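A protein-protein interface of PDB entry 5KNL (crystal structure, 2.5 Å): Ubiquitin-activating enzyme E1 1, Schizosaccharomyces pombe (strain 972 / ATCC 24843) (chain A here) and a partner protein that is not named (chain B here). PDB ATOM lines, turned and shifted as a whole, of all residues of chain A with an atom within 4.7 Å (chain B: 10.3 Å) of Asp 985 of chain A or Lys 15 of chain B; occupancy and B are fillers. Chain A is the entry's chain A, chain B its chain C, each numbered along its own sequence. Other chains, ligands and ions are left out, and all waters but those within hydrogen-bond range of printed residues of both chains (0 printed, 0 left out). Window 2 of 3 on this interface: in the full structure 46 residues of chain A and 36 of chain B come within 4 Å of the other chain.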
ATOM      1  N   LEU A 929      -5.628  19.537  25.524  1.00  0.00           N
ATOM      2  CA  LEU A 929      -7.041  19.888  25.420  1.00  0.00           C
ATOM      3  C   LEU A 929      -7.838  19.215  26.531  1.00  0.00           C
ATOM      4  O   LEU A 929      -7.688  18.017  26.767  1.00  0.00           O
ATOM      5  CB  LEU A 929      -7.599  19.472  24.058  1.00  0.00           C
ATOM      6  CG  LEU A 929      -6.911  20.044  22.816  1.00  0.00           C
ATOM      7  CD1 LEU A 929      -7.342  19.279  21.575  1.00  0.00           C
ATOM      8  CD2 LEU A 929      -7.221  21.524  22.665  1.00  0.00           C
ATOM      9  N   GLU A 930      -8.686  19.983  27.207  1.00  0.00           N
ATOM     10  CA  GLU A 930      -9.553  19.419  28.235  1.00  0.00           C
ATOM     11  C   GLU A 930     -10.838  18.901  27.599  1.00  0.00           C
ATOM     12  O   GLU A 930     -11.554  19.642  26.925  1.00  0.00           O
ATOM     13  CB  GLU A 930      -9.873  20.451  29.326  1.00  0.00           C
ATOM     14  CG  GLU A 930     -10.428  21.783  28.824  1.00  0.00           C
ATOM     15  CD  GLU A 930     -10.906  22.683  29.952  1.00  0.00           C
ATOM     16  OE1 GLU A 930     -11.373  22.156  30.985  1.00  0.00           O
ATOM     17  OE2 GLU A 930     -10.820  23.921  29.803  1.00  0.00           O
ATOM     18  N   THR A 932     -14.241  18.490  27.512  1.00  0.00           N
ATOM     19  CA  THR A 932     -15.388  19.087  28.184  1.00  0.00           C
ATOM     20  C   THR A 932     -16.622  18.200  28.078  1.00  0.00           C
ATOM     21  O   THR A 932     -17.542  18.302  28.890  1.00  0.00           O
ATOM     22  CB  THR A 932     -15.725  20.468  27.597  1.00  0.00           C
ATOM     23  OG1 THR A 932     -16.089  20.331  26.218  1.00  0.00           O
ATOM     24  CG2 THR A 932     -14.533  21.407  27.719  1.00  0.00           C
ATOM     25  N   MET A 933     -16.638  17.331  27.075  1.00  0.00           N
ATOM     26  CA  MET A 933     -17.790  16.477  26.828  1.00  0.00           C
ATOM     27  C   MET A 933     -17.404  15.305  25.936  1.00  0.00           C
ATOM     28  O   MET A 933     -16.583  15.451  25.031  1.00  0.00           O
ATOM     29  CB  MET A 933     -18.918  17.285  26.189  1.00  0.00           C
ATOM     30  CG  MET A 933     -20.220  16.526  26.036  1.00  0.00           C
ATOM     31  SD  MET A 933     -21.640  17.622  25.845  1.00  0.00           S
ATOM     32  CE  MET A 933     -20.989  18.818  24.681  1.00  0.00           C
ATOM     33  N   PHE A 945     -20.171  19.283  32.961  1.00  0.00           N
ATOM     34  CA  PHE A 945     -21.266  19.933  33.676  1.00  0.00           C
ATOM     35  C   PHE A 945     -22.154  18.917  34.394  1.00  0.00           C
ATOM     36  O   PHE A 945     -23.056  19.296  35.142  1.00  0.00           O
ATOM     37  CB  PHE A 945     -22.111  20.789  32.720  1.00  0.00           C
ATOM     38  CG  PHE A 945     -22.678  20.034  31.541  1.00  0.00           C
ATOM     39  CD1 PHE A 945     -23.708  19.121  31.709  1.00  0.00           C
ATOM     40  CD2 PHE A 945     -22.197  20.262  30.261  1.00  0.00           C
ATOM     41  CE1 PHE A 945     -24.234  18.437  30.627  1.00  0.00           C
ATOM     42  CE2 PHE A 945     -22.720  19.582  29.175  1.00  0.00           C
ATOM     43  CZ  PHE A 945     -23.740  18.669  29.359  1.00  0.00           C
ATOM     44  N   CYS A 983     -16.047  17.253  22.631  1.00  0.00           N
ATOM     45  CA  CYS A 983     -15.888  18.700  22.583  1.00  0.00           C
ATOM     46  C   CYS A 983     -14.683  19.063  23.439  1.00  0.00           C
ATOM     47  O   CYS A 983     -14.557  18.594  24.571  1.00  0.00           O
ATOM     48  CB  CYS A 983     -17.149  19.408  23.079  1.00  0.00           C
ATOM     49  SG  CYS A 983     -18.642  18.982  22.154  1.00  0.00           S
ATOM     50  N   CYS A 984     -13.801  19.892  22.892  1.00  0.00           N
ATOM     51  CA  CYS A 984     -12.526  20.187  23.532  1.00  0.00           C
ATOM     52  C   CYS A 984     -12.222  21.676  23.561  1.00  0.00           C
ATOM     53  O   CYS A 984     -12.321  22.360  22.542  1.00  0.00           O
ATOM     54  CB  CYS A 984     -11.399  19.448  22.814  1.00  0.00           C
ATOM     55  SG  CYS A 984     -11.411  17.668  23.078  1.00  0.00           S
ATOM     56  N   ASP A 985     -11.842  22.163  24.738  1.00  0.00           N
ATOM     57  CA  ASP A 985     -11.403  23.541  24.905  1.00  0.00           C
ATOM     58  C   ASP A 985      -9.901  23.577  25.151  1.00  0.00           C
ATOM     59  O   ASP A 985      -9.377  22.797  25.944  1.00  0.00           O
ATOM     60  CB  ASP A 985     -12.142  24.208  26.068  1.00  0.00           C
ATOM     61  CG  ASP A 985     -13.637  24.300  25.837  1.00  0.00           C
ATOM     62  OD1 ASP A 985     -14.167  23.512  25.025  1.00  0.00           O
ATOM     63  OD2 ASP A 985     -14.285  25.159  26.471  1.00  0.00           O
ATOM     64  N   ASP A 986      -9.209  24.477  24.462  1.00  0.00           N
ATOM     65  CA  ASP A 986      -7.794  24.706  24.727  1.00  0.00           C
ATOM     66  C   ASP A 986      -7.666  25.569  25.978  1.00  0.00           C
ATOM     67  O   ASP A 986      -8.615  26.252  26.363  1.00  0.00           O
ATOM     68  CB  ASP A 986      -7.099  25.365  23.530  1.00  0.00           C
ATOM     69  CG  ASP A 986      -7.893  26.524  22.947  1.00  0.00           C
ATOM     70  OD1 ASP A 986      -8.689  27.142  23.684  1.00  0.00           O
ATOM     71  OD2 ASP A 986      -7.718  26.814  21.746  1.00  0.00           O
ATOM     72  N   ALA A 987      -6.502  25.526  26.618  1.00  0.00           N
ATOM     73  CA  ALA A 987      -6.272  26.295  27.836  1.00  0.00           C
ATOM     74  C   ALA A 987      -6.425  27.792  27.579  1.00  0.00           C
ATOM     75  O   ALA A 987      -5.446  28.537  27.591  1.00  0.00           O
ATOM     76  CB  ALA A 987      -4.892  25.993  28.399  1.00  0.00           C
ATOM     77  N   GLY A 989     -10.306  29.035  27.175  1.00  0.00           N
ATOM     78  CA  GLY A 989     -11.704  29.225  27.524  1.00  0.00           C
ATOM     79  C   GLY A 989     -12.668  28.829  26.421  1.00  0.00           C
ATOM     80  O   GLY A 989     -13.791  28.407  26.695  1.00  0.00           O
ATOM     81  N   GLU A 990     -12.229  28.964  25.171  1.00  0.00           N
ATOM     82  CA  GLU A 990     -13.092  28.713  24.019  1.00  0.00           C
ATOM     83  C   GLU A 990     -12.896  27.305  23.454  1.00  0.00           C
ATOM     84  O   GLU A 990     -11.850  26.686  23.645  1.00  0.00           O
ATOM     85  CB  GLU A 990     -12.843  29.764  22.935  1.00  0.00           C
ATOM     86  CG  GLU A 990     -13.269  31.168  23.349  1.00  0.00           C
ATOM     87  CD  GLU A 990     -13.123  32.184  22.234  1.00  0.00           C
ATOM     88  OE1 GLU A 990     -12.640  31.812  21.143  1.00  0.00           O
ATOM     89  OE2 GLU A 990     -13.492  33.358  22.450  1.00  0.00           O
ATOM     90  N   ASP A 991     -13.919  26.815  22.757  1.00  0.00           N
ATOM     91  CA  ASP A 991     -13.950  25.439  22.263  1.00  0.00           C
ATOM     92  C   ASP A 991     -13.212  25.253  20.936  1.00  0.00           C
ATOM     93  O   ASP A 991     -13.042  26.198  20.165  1.00  0.00           O
ATOM     94  CB  ASP A 991     -15.409  24.983  22.121  1.00  0.00           C
ATOM     95  CG  ASP A 991     -15.637  24.100  20.906  1.00  0.00           C
ATOM     96  OD1 ASP A 991     -15.946  24.642  19.823  1.00  0.00           O
ATOM     97  OD2 ASP A 991     -15.511  22.864  21.033  1.00  0.00           O
ATOM     98  N   VAL A 992     -12.777  24.020  20.690  1.00  0.00           N
ATOM     99  CA  VAL A 992     -12.089  23.648  19.458  1.00  0.00           C
ATOM    100  C   VAL A 992     -12.532  22.253  19.022  1.00  0.00           C
ATOM    101  O   VAL A 992     -12.235  21.264  19.692  1.00  0.00           O
ATOM    102  CB  VAL A 992     -10.553  23.665  19.632  1.00  0.00           C
ATOM    103  CG1 VAL A 992      -9.854  23.252  18.339  1.00  0.00           C
ATOM    104  CG2 VAL A 992     -10.078  25.040  20.078  1.00  0.00           C
ATOM    105  N   GLU B   7     -26.204  15.332  15.699  1.00  0.00           N
ATOM    106  CA  GLU B   7     -25.675  14.941  17.001  1.00  0.00           C
ATOM    107  C   GLU B   7     -24.694  15.973  17.544  1.00  0.00           C
ATOM    108  O   GLU B   7     -24.720  16.295  18.731  1.00  0.00           O
ATOM    109  CB  GLU B   7     -24.994  13.575  16.900  1.00  0.00           C
ATOM    110  CG  GLU B   7     -25.945  12.437  16.555  1.00  0.00           C
ATOM    111  CD  GLU B   7     -25.227  11.214  16.013  1.00  0.00           C
ATOM    112  OE1 GLU B   7     -24.183  10.831  16.582  1.00  0.00           O
ATOM    113  OE2 GLU B   7     -25.709  10.633  15.017  1.00  0.00           O
ATOM    114  N   GLN B   8     -23.835  16.493  16.674  1.00  0.00           N
ATOM    115  CA  GLN B   8     -22.831  17.467  17.083  1.00  0.00           C
ATOM    116  C   GLN B   8     -23.478  18.764  17.547  1.00  0.00           C
ATOM    117  O   GLN B   8     -23.051  19.362  18.534  1.00  0.00           O
ATOM    118  CB  GLN B   8     -21.861  17.761  15.936  1.00  0.00           C
ATOM    119  CG  GLN B   8     -20.981  16.587  15.540  1.00  0.00           C
ATOM    120  CD  GLN B   8     -19.932  16.967  14.511  1.00  0.00           C
ATOM    121  OE1 GLN B   8     -19.440  18.097  14.496  1.00  0.00           O
ATOM    122  NE2 GLN B   8     -19.589  16.026  13.639  1.00  0.00           N
ATOM    123  N   LEU B   9     -24.510  19.196  16.832  1.00  0.00           N
ATOM    124  CA  LEU B   9     -25.171  20.457  17.139  1.00  0.00           C
ATOM    125  C   LEU B   9     -25.910  20.382  18.471  1.00  0.00           C
ATOM    126  O   LEU B   9     -25.924  21.348  19.234  1.00  0.00           O
ATOM    127  CB  LEU B   9     -26.138  20.836  16.015  1.00  0.00           C
ATOM    128  CG  LEU B   9     -26.914  22.144  16.187  1.00  0.00           C
ATOM    129  CD1 LEU B   9     -25.963  23.323  16.350  1.00  0.00           C
ATOM    130  CD2 LEU B   9     -27.845  22.371  15.005  1.00  0.00           C
ATOM    131  N   LEU B  10     -26.521  19.234  18.752  1.00  0.00           N
ATOM    132  CA  LEU B  10     -27.262  19.056  19.996  1.00  0.00           C
ATOM    133  C   LEU B  10     -26.326  19.067  21.197  1.00  0.00           C
ATOM    134  O   LEU B  10     -26.679  19.579  22.260  1.00  0.00           O
ATOM    135  CB  LEU B  10     -28.064  17.754  19.968  1.00  0.00           C
ATOM    136  CG  LEU B  10     -29.339  17.755  19.122  1.00  0.00           C
ATOM    137  CD1 LEU B  10     -29.944  16.363  19.070  1.00  0.00           C
ATOM    138  CD2 LEU B  10     -30.360  18.749  19.671  1.00  0.00           C
ATOM    139  N   ARG B  11     -25.136  18.503  21.028  1.00  0.00           N
ATOM    140  CA  ARG B  11     -24.140  18.516  22.091  1.00  0.00           C
ATOM    141  C   ARG B  11     -23.772  19.946  22.459  1.00  0.00           C
ATOM    142  O   ARG B  11     -23.884  20.342  23.618  1.00  0.00           O
ATOM    143  CB  ARG B  11     -22.888  17.739  21.681  1.00  0.00           C
ATOM    144  CG  ARG B  11     -23.050  16.232  21.740  1.00  0.00           C
ATOM    145  CD  ARG B  11     -21.741  15.517  21.464  1.00  0.00           C
ATOM    146  NE  ARG B  11     -21.806  14.693  20.256  1.00  0.00           N
ATOM    147  CZ  ARG B  11     -21.110  14.907  19.141  1.00  0.00           C
ATOM    148  NH1 ARG B  11     -20.259  15.923  19.043  1.00  0.00           N
ATOM    149  NH2 ARG B  11     -21.260  14.086  18.111  1.00  0.00           N
ATOM    150  N   LYS B  12     -23.335  20.714  21.466  1.00  0.00           N
ATOM    151  CA  LYS B  12     -22.910  22.092  21.688  1.00  0.00           C
ATOM    152  C   LYS B  12     -24.037  22.934  22.276  1.00  0.00           C
ATOM    153  O   LYS B  12     -23.799  23.797  23.119  1.00  0.00           O
ATOM    154  CB  LYS B  12     -22.418  22.712  20.378  1.00  0.00           C
ATOM    155  CG  LYS B  12     -21.229  21.988  19.760  1.00  0.00           C
ATOM    156  CD  LYS B  12     -20.010  22.020  20.673  1.00  0.00           C
ATOM    157  CE  LYS B  12     -18.791  21.407  20.002  1.00  0.00           C
ATOM    158  NZ  LYS B  12     -19.043  20.003  19.565  1.00  0.00           N
ATOM    159  N   GLN B  13     -25.264  22.681  21.831  1.00  0.00           N
ATOM    160  CA  GLN B  13     -26.424  23.408  22.335  1.00  0.00           C
ATOM    161  C   GLN B  13     -26.797  22.949  23.743  1.00  0.00           C
ATOM    162  O   GLN B  13     -27.237  23.752  24.566  1.00  0.00           O
ATOM    163  CB  GLN B  13     -27.611  23.243  21.387  1.00  0.00           C
ATOM    164  CG  GLN B  13     -27.452  24.016  20.084  1.00  0.00           C
ATOM    165  CD  GLN B  13     -28.612  23.816  19.128  1.00  0.00           C
ATOM    166  OE1 GLN B  13     -29.387  22.869  19.259  1.00  0.00           O
ATOM    167  NE2 GLN B  13     -28.738  24.715  18.158  1.00  0.00           N
ATOM    168  N   LEU B  14     -26.623  21.659  24.016  1.00  0.00           N
ATOM    169  CA  LEU B  14     -26.867  21.125  25.353  1.00  0.00           C
ATOM    170  C   LEU B  14     -25.839  21.675  26.330  1.00  0.00           C
ATOM    171  O   LEU B  14     -26.150  21.965  27.485  1.00  0.00           O
ATOM    172  CB  LEU B  14     -26.811  19.595  25.350  1.00  0.00           C
ATOM    173  CG  LEU B  14     -27.107  18.911  26.688  1.00  0.00           C
ATOM    174  CD1 LEU B  14     -28.550  19.135  27.110  1.00  0.00           C
ATOM    175  CD2 LEU B  14     -26.793  17.425  26.621  1.00  0.00           C
ATOM    176  N   LYS B  15     -24.608  21.808  25.850  1.00  0.00           N
ATOM    177  CA  LYS B  15     -23.518  22.329  26.660  1.00  0.00           C
ATOM    178  C   LYS B  15     -23.759  23.792  27.007  1.00  0.00           C
ATOM    179  O   LYS B  15     -23.621  24.192  28.161  1.00  0.00           O
ATOM    180  CB  LYS B  15     -22.190  22.159  25.921  1.00  0.00           C
ATOM    181  CG  LYS B  15     -20.957  22.509  26.733  1.00  0.00           C
ATOM    182  CD  LYS B  15     -19.690  22.131  25.977  1.00  0.00           C
ATOM    183  CE  LYS B  15     -18.562  23.121  26.222  1.00  0.00           C
ATOM    184  NZ  LYS B  15     -17.387  22.845  25.347  1.00  0.00           N
ATOM    185  N   GLU B  16     -24.137  24.583  26.007  1.00  0.00           N
ATOM    186  CA  GLU B  16     -24.341  26.017  26.195  1.00  0.00           C
ATOM    187  C   GLU B  16     -25.523  26.331  27.108  1.00  0.00           C
ATOM    188  O   GLU B  16     -25.433  27.218  27.956  1.00  0.00           O
ATOM    189  CB  GLU B  16     -24.541  26.708  24.846  1.00  0.00           C
ATOM    190  CG  GLU B  16     -23.257  26.903  24.061  1.00  0.00           C
ATOM    191  CD  GLU B  16     -23.477  27.651  22.761  1.00  0.00           C
ATOM    192  OE1 GLU B  16     -24.647  27.930  22.425  1.00  0.00           O
ATOM    193  OE2 GLU B  16     -22.478  27.960  22.077  1.00  0.00           O
ATOM    194  N   ILE B  17     -26.629  25.615  26.937  1.00  0.00           N
ATOM    195  CA  ILE B  17     -27.802  25.850  27.770  1.00  0.00           C
ATOM    196  C   ILE B  17     -27.510  25.378  29.188  1.00  0.00           C
ATOM    197  O   ILE B  17     -27.933  26.009  30.157  1.00  0.00           O
ATOM    198  CB  ILE B  17     -29.058  25.140  27.204  1.00  0.00           C
ATOM    199  CG1 ILE B  17     -29.649  25.981  26.068  1.00  0.00           C
ATOM    200  CG2 ILE B  17     -30.107  24.905  28.300  1.00  0.00           C
ATOM    201  CD1 ILE B  17     -30.888  25.395  25.412  1.00  0.00           C
ATOM    202  N   GLN B  18     -26.775  24.276  29.303  1.00  0.00           N
ATOM    203  CA  GLN B  18     -26.388  23.742  30.605  1.00  0.00           C
ATOM    204  C   GLN B  18     -25.034  24.309  31.024  1.00  0.00           C
ATOM    205  O   GLN B  18     -24.220  23.617  31.637  1.00  0.00           O
ATOM    206  CB  GLN B  18     -26.348  22.211  30.572  1.00  0.00           C
ATOM    207  CG  GLN B  18     -26.439  21.549  31.945  1.00  0.00           C
ATOM    208  CD  GLN B  18     -27.694  21.941  32.707  1.00  0.00           C
ATOM    209  OE1 GLN B  18     -28.718  22.271  32.110  1.00  0.00           O
ATOM    210  NE2 GLN B  18     -27.615  21.911  34.033  1.00  0.00           N
ATOM    211  N   LYS B  19     -24.800  25.571  30.677  1.00  0.00           N
ATOM    212  CA  LYS B  19     -23.598  26.283  31.091  1.00  0.00           C
ATOM    213  C   LYS B  19     -24.039  27.546  31.823  1.00  0.00           C
ATOM    214  O   LYS B  19     -23.738  27.732  33.003  1.00  0.00           O
ATOM    215  CB  LYS B  19     -22.727  26.624  29.877  1.00  0.00           C
ATOM    216  CG  LYS B  19     -21.511  27.490  30.162  1.00  0.00           C
ATOM    217  CD  LYS B  19     -20.603  26.845  31.199  1.00  0.00           C
ATOM    218  CE  LYS B  19     -19.368  27.689  31.464  1.00  0.00           C
ATOM    219  NZ  LYS B  19     -18.585  27.180  32.624  1.00  0.00           N
ATOM    220  N   ASN B  20     -24.763  28.402  31.105  1.00  0.00           N
ATOM    221  CA  ASN B  20     -25.373  29.597  31.676  1.00  0.00           C
ATOM    222  C   ASN B  20     -26.893  29.530  31.528  1.00  0.00           C
ATOM    223  O   ASN B  20     -27.477  30.271  30.736  1.00  0.00           O
ATOM    224  CB  ASN B  20     -24.818  30.857  31.005  1.00  0.00           C
ATOM    225  CG  ASN B  20     -24.673  30.706  29.503  1.00  0.00           C
ATOM    226  OD1 ASN B  20     -25.474  30.035  28.853  1.00  0.00           O
ATOM    227  ND2 ASN B  20     -23.641  31.328  28.945  1.00  0.00           N
ATOM    228  N   PRO B  21     -27.539  28.635  32.294  1.00  0.00           N
ATOM    229  CA  PRO B  21     -28.973  28.368  32.118  1.00  0.00           C
ATOM    230  C   PRO B  21     -29.858  29.599  32.329  1.00  0.00           C
ATOM    231  O   PRO B  21     -29.858  30.156  33.427  1.00  0.00           O
ATOM    232  CB  PRO B  21     -29.264  27.308  33.188  1.00  0.00           C
ATOM    233  CG  PRO B  21     -28.199  27.488  34.206  1.00  0.00           C
ATOM    234  CD  PRO B  21     -26.982  27.899  33.442  1.00  0.00           C
ATOM    235  N   PRO B  22     -30.602  30.022  31.291  1.00  0.00           N
ATOM    236  CA  PRO B  22     -31.530  31.146  31.472  1.00  0.00           C
ATOM    237  C   PRO B  22     -32.654  30.805  32.444  1.00  0.00           C
ATOM    238  O   PRO B  22     -33.305  29.770  32.297  1.00  0.00           O
ATOM    239  CB  PRO B  22     -32.069  31.386  30.060  1.00  0.00           C
ATOM    240  CG  PRO B  22     -31.921  30.081  29.385  1.00  0.00           C
ATOM    241  CD  PRO B  22     -30.662  29.489  29.919  1.00  0.00           C
ATOM    242  N   VAL B  27     -33.147  22.455  31.891  1.00  0.00           N
ATOM    243  CA  VAL B  27     -33.014  21.548  30.755  1.00  0.00           C
ATOM    244  C   VAL B  27     -32.054  20.406  31.063  1.00  0.00           C
ATOM    245  O   VAL B  27     -30.963  20.613  31.594  1.00  0.00           O
ATOM    246  CB  VAL B  27     -32.520  22.297  29.499  1.00  0.00           C
ATOM    247  CG1 VAL B  27     -32.303  21.332  28.342  1.00  0.00           C
ATOM    248  CG2 VAL B  27     -33.511  23.380  29.106  1.00  0.00           C
ATOM    249  N   GLY B  28     -32.484  19.198  30.723  1.00  0.00           N
ATOM    250  CA  GLY B  28     -31.675  18.007  30.893  1.00  0.00           C
ATOM    251  C   GLY B  28     -32.167  16.940  29.942  1.00  0.00           C
ATOM    252  O   GLY B  28     -33.145  17.152  29.225  1.00  0.00           O
ATOM    253  N   LEU B  29     -31.495  15.795  29.928  1.00  0.00           N
ATOM    254  CA  LEU B  29     -31.915  14.681  29.089  1.00  0.00           C
ATOM    255  C   LEU B  29     -32.837  13.748  29.862  1.00  0.00           C
ATOM    256  O   LEU B  29     -32.613  13.485  31.043  1.00  0.00           O
ATOM    257  CB  LEU B  29     -30.699  13.903  28.575  1.00  0.00           C
ATOM    258  CG  LEU B  29     -29.602  14.711  27.875  1.00  0.00           C
ATOM    259  CD1 LEU B  29     -28.476  13.795  27.409  1.00  0.00           C
ATOM    260  CD2 LEU B  29     -30.165  15.506  26.708  1.00  0.00           C
ATOM    261  N   ILE B  35     -29.386  12.144  23.335  1.00  0.00           N
ATOM    262  CA  ILE B  35     -29.371  13.602  23.415  1.00  0.00           C
ATOM    263  C   ILE B  35     -30.472  14.209  22.550  1.00  0.00           C
ATOM    264  O   ILE B  35     -30.596  15.430  22.457  1.00  0.00           O
ATOM    265  CB  ILE B  35     -28.009  14.187  22.979  1.00  0.00           C
ATOM    266  CG1 ILE B  35     -27.723  13.837  21.512  1.00  0.00           C
ATOM    267  CG2 ILE B  35     -26.907  13.683  23.903  1.00  0.00           C
ATOM    268  CD1 ILE B  35     -26.375  14.310  20.998  1.00  0.00           C
ATOM    269  N   TRP B  38     -34.839  15.649  25.207  1.00  0.00           N
ATOM    270  CA  TRP B  38     -34.677  16.524  26.359  1.00  0.00           C
ATOM    271  C   TRP B  38     -35.966  16.572  27.164  1.00  0.00           C
ATOM    272  O   TRP B  38     -37.059  16.501  26.602  1.00  0.00           O
ATOM    273  CB  TRP B  38     -34.294  17.940  25.922  1.00  0.00           C
ATOM    274  CG  TRP B  38     -33.010  18.044  25.158  1.00  0.00           C
ATOM    275  CD1 TRP B  38     -32.305  17.026  24.586  1.00  0.00           C
ATOM    276  CD2 TRP B  38     -32.282  19.243  24.875  1.00  0.00           C
ATOM    277  NE1 TRP B  38     -31.183  17.518  23.966  1.00  0.00           N
ATOM    278  CE2 TRP B  38     -31.146  18.877  24.131  1.00  0.00           C
ATOM    279  CE3 TRP B  38     -32.482  20.592  25.182  1.00  0.00           C
ATOM    280  CZ2 TRP B  38     -30.211  19.810  23.689  1.00  0.00           C
ATOM    281  CZ3 TRP B  38     -31.553  21.516  24.742  1.00  0.00           C
ATOM    282  CH2 TRP B  38     -30.432  21.121  24.005  1.00  0.00           C
ATOM    283  N   PRO B 117     -32.597  25.870  20.948  1.00  0.00           N
ATOM    284  CA  PRO B 117     -33.640  25.400  21.868  1.00  0.00           C
ATOM    285  C   PRO B 117     -34.019  26.459  22.898  1.00  0.00           C
ATOM    286  O   PRO B 117     -35.152  26.478  23.374  1.00  0.00           O
ATOM    287  CB  PRO B 117     -33.003  24.180  22.552  1.00  0.00           C
ATOM    288  CG  PRO B 117     -31.637  24.010  21.949  1.00  0.00           C
ATOM    289  CD  PRO B 117     -31.559  24.851  20.725  1.00  0.00           C
ATOM    290  N   GLU B 118     -33.075  27.332  23.229  1.00  0.00           N
ATOM    291  CA  GLU B 118     -33.338  28.425  24.155  1.00  0.00           C
ATOM    292  C   GLU B 118     -34.343  29.404  23.555  1.00  0.00           C
ATOM    293  O   GLU B 118     -35.264  29.854  24.234  1.00  0.00           O
ATOM    294  CB  GLU B 118     -32.037  29.147  24.512  1.00  0.00           C
ATOM    295  CG  GLU B 118     -32.215  30.312  25.475  1.00  0.00           C
ATOM    296  CD  GLU B 118     -30.895  30.854  25.995  1.00  0.00           C
ATOM    297  OE1 GLU B 118     -29.837  30.274  25.665  1.00  0.00           O
ATOM    298  OE2 GLU B 118     -30.917  31.865  26.731  1.00  0.00           O
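The side-chain sulfur (SG) of Cys 983 of chain A lies within hydrogen-bond range of the side-chain amino group (NZ) of Lys 12 of chain B, 2.8 Å away.
OG1 of Thr 932 of chain A lies within hydrogen-bond range of NZ of Lys 15 of chain B (3.0 Å).
The side-chain carboxylate (OD1) of Asp 985 of chain A lies within salt-bridge range of the side-chain amino group (NZ) of Lys 15 of chain B (3.3 Å).
Of the 23 printed residues of chain B, 4 touch a printed residue of chain A.
Along chain B the printed residues that touch a printed residue of chain A span positions 11 to 18.
Among the printed residues, 8 pairs touch across the chains.
CE of Met 933 of chain A touches O of Arg 11 of chain B (3.4 Å).
Met 933 of chain A touches Lys 15 of chain B (CE to CB, 3.8 Å).
Lys 15 of chain B touches Phe 945 of chain A.
Phe 945 of chain A touches Gln 18 of chain B.
Lys 12 of chain B touches Asp 991 of chain A.
N of Glu 930 of chain A lies within hydrogen-bond range of O of Asp 985 of chain A, 3.2 Å away.
The side-chain hydroxyl (OG1) of Thr 932 of chain A is in hydrogen-bond range of the backbone carbonyl oxygen (O) of Cys 983 of chain A, at 2.8 Å.
OE1 of Gln 18 of chain B lies close to O of Val 27 of chain B, 2.8 Å away.
The backbone carbonyl oxygen of Met 933 of chain A sits at hydrogen-bond distance from the backbone NH of Cys 983 of chain A, at 3.0 Å.
Of chain A, only Thr 932, Met 933, Phe 945 and Asp 985 come within 4 Å of Lys 15 of chain B.
No residue of chain B comes within 4 Å of Leu 929 of chain A.
Of chain B, only Lys 15 comes within 4 Å of Thr 932 of chain A.
No residue of chain B comes within 4 Å of Asp 986 of chain A.
No residue of chain B comes within 4 Å of Gly 989 of chain A.
Printed residues of chain B within 4 Å of Asp 991 of chain A: Lys 12 (3.7 Å).
Printed residues of chain A within 4 Å of Arg 11 of chain B: Met 933.
Of the printed residues of chain A, Gln 18 of chain B touches Phe 945.
Of the printed residues of chain B, Phe 945 of chain A touches Lys 15 and Gln 18.
Of the printed residues of chain B, Cys 983 of chain A touches Lys 12 (2.8 Å).
Of the printed residues of chain B, Met 933 of chain A touches Arg 11 and Lys 15.
Asn 20 of chain B touches none of the printed residues of chain A.
Leu 9 of chain B touches none of the printed residues of chain A.
The nearest residue of chain B that does not touch Asp 985 of chain A is Lys 12 of chain B (7.1 Å).
The nearest printed residue of chain A that does not touch Gln 18 of chain B is Met 933 of chain A (8.1 Å).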
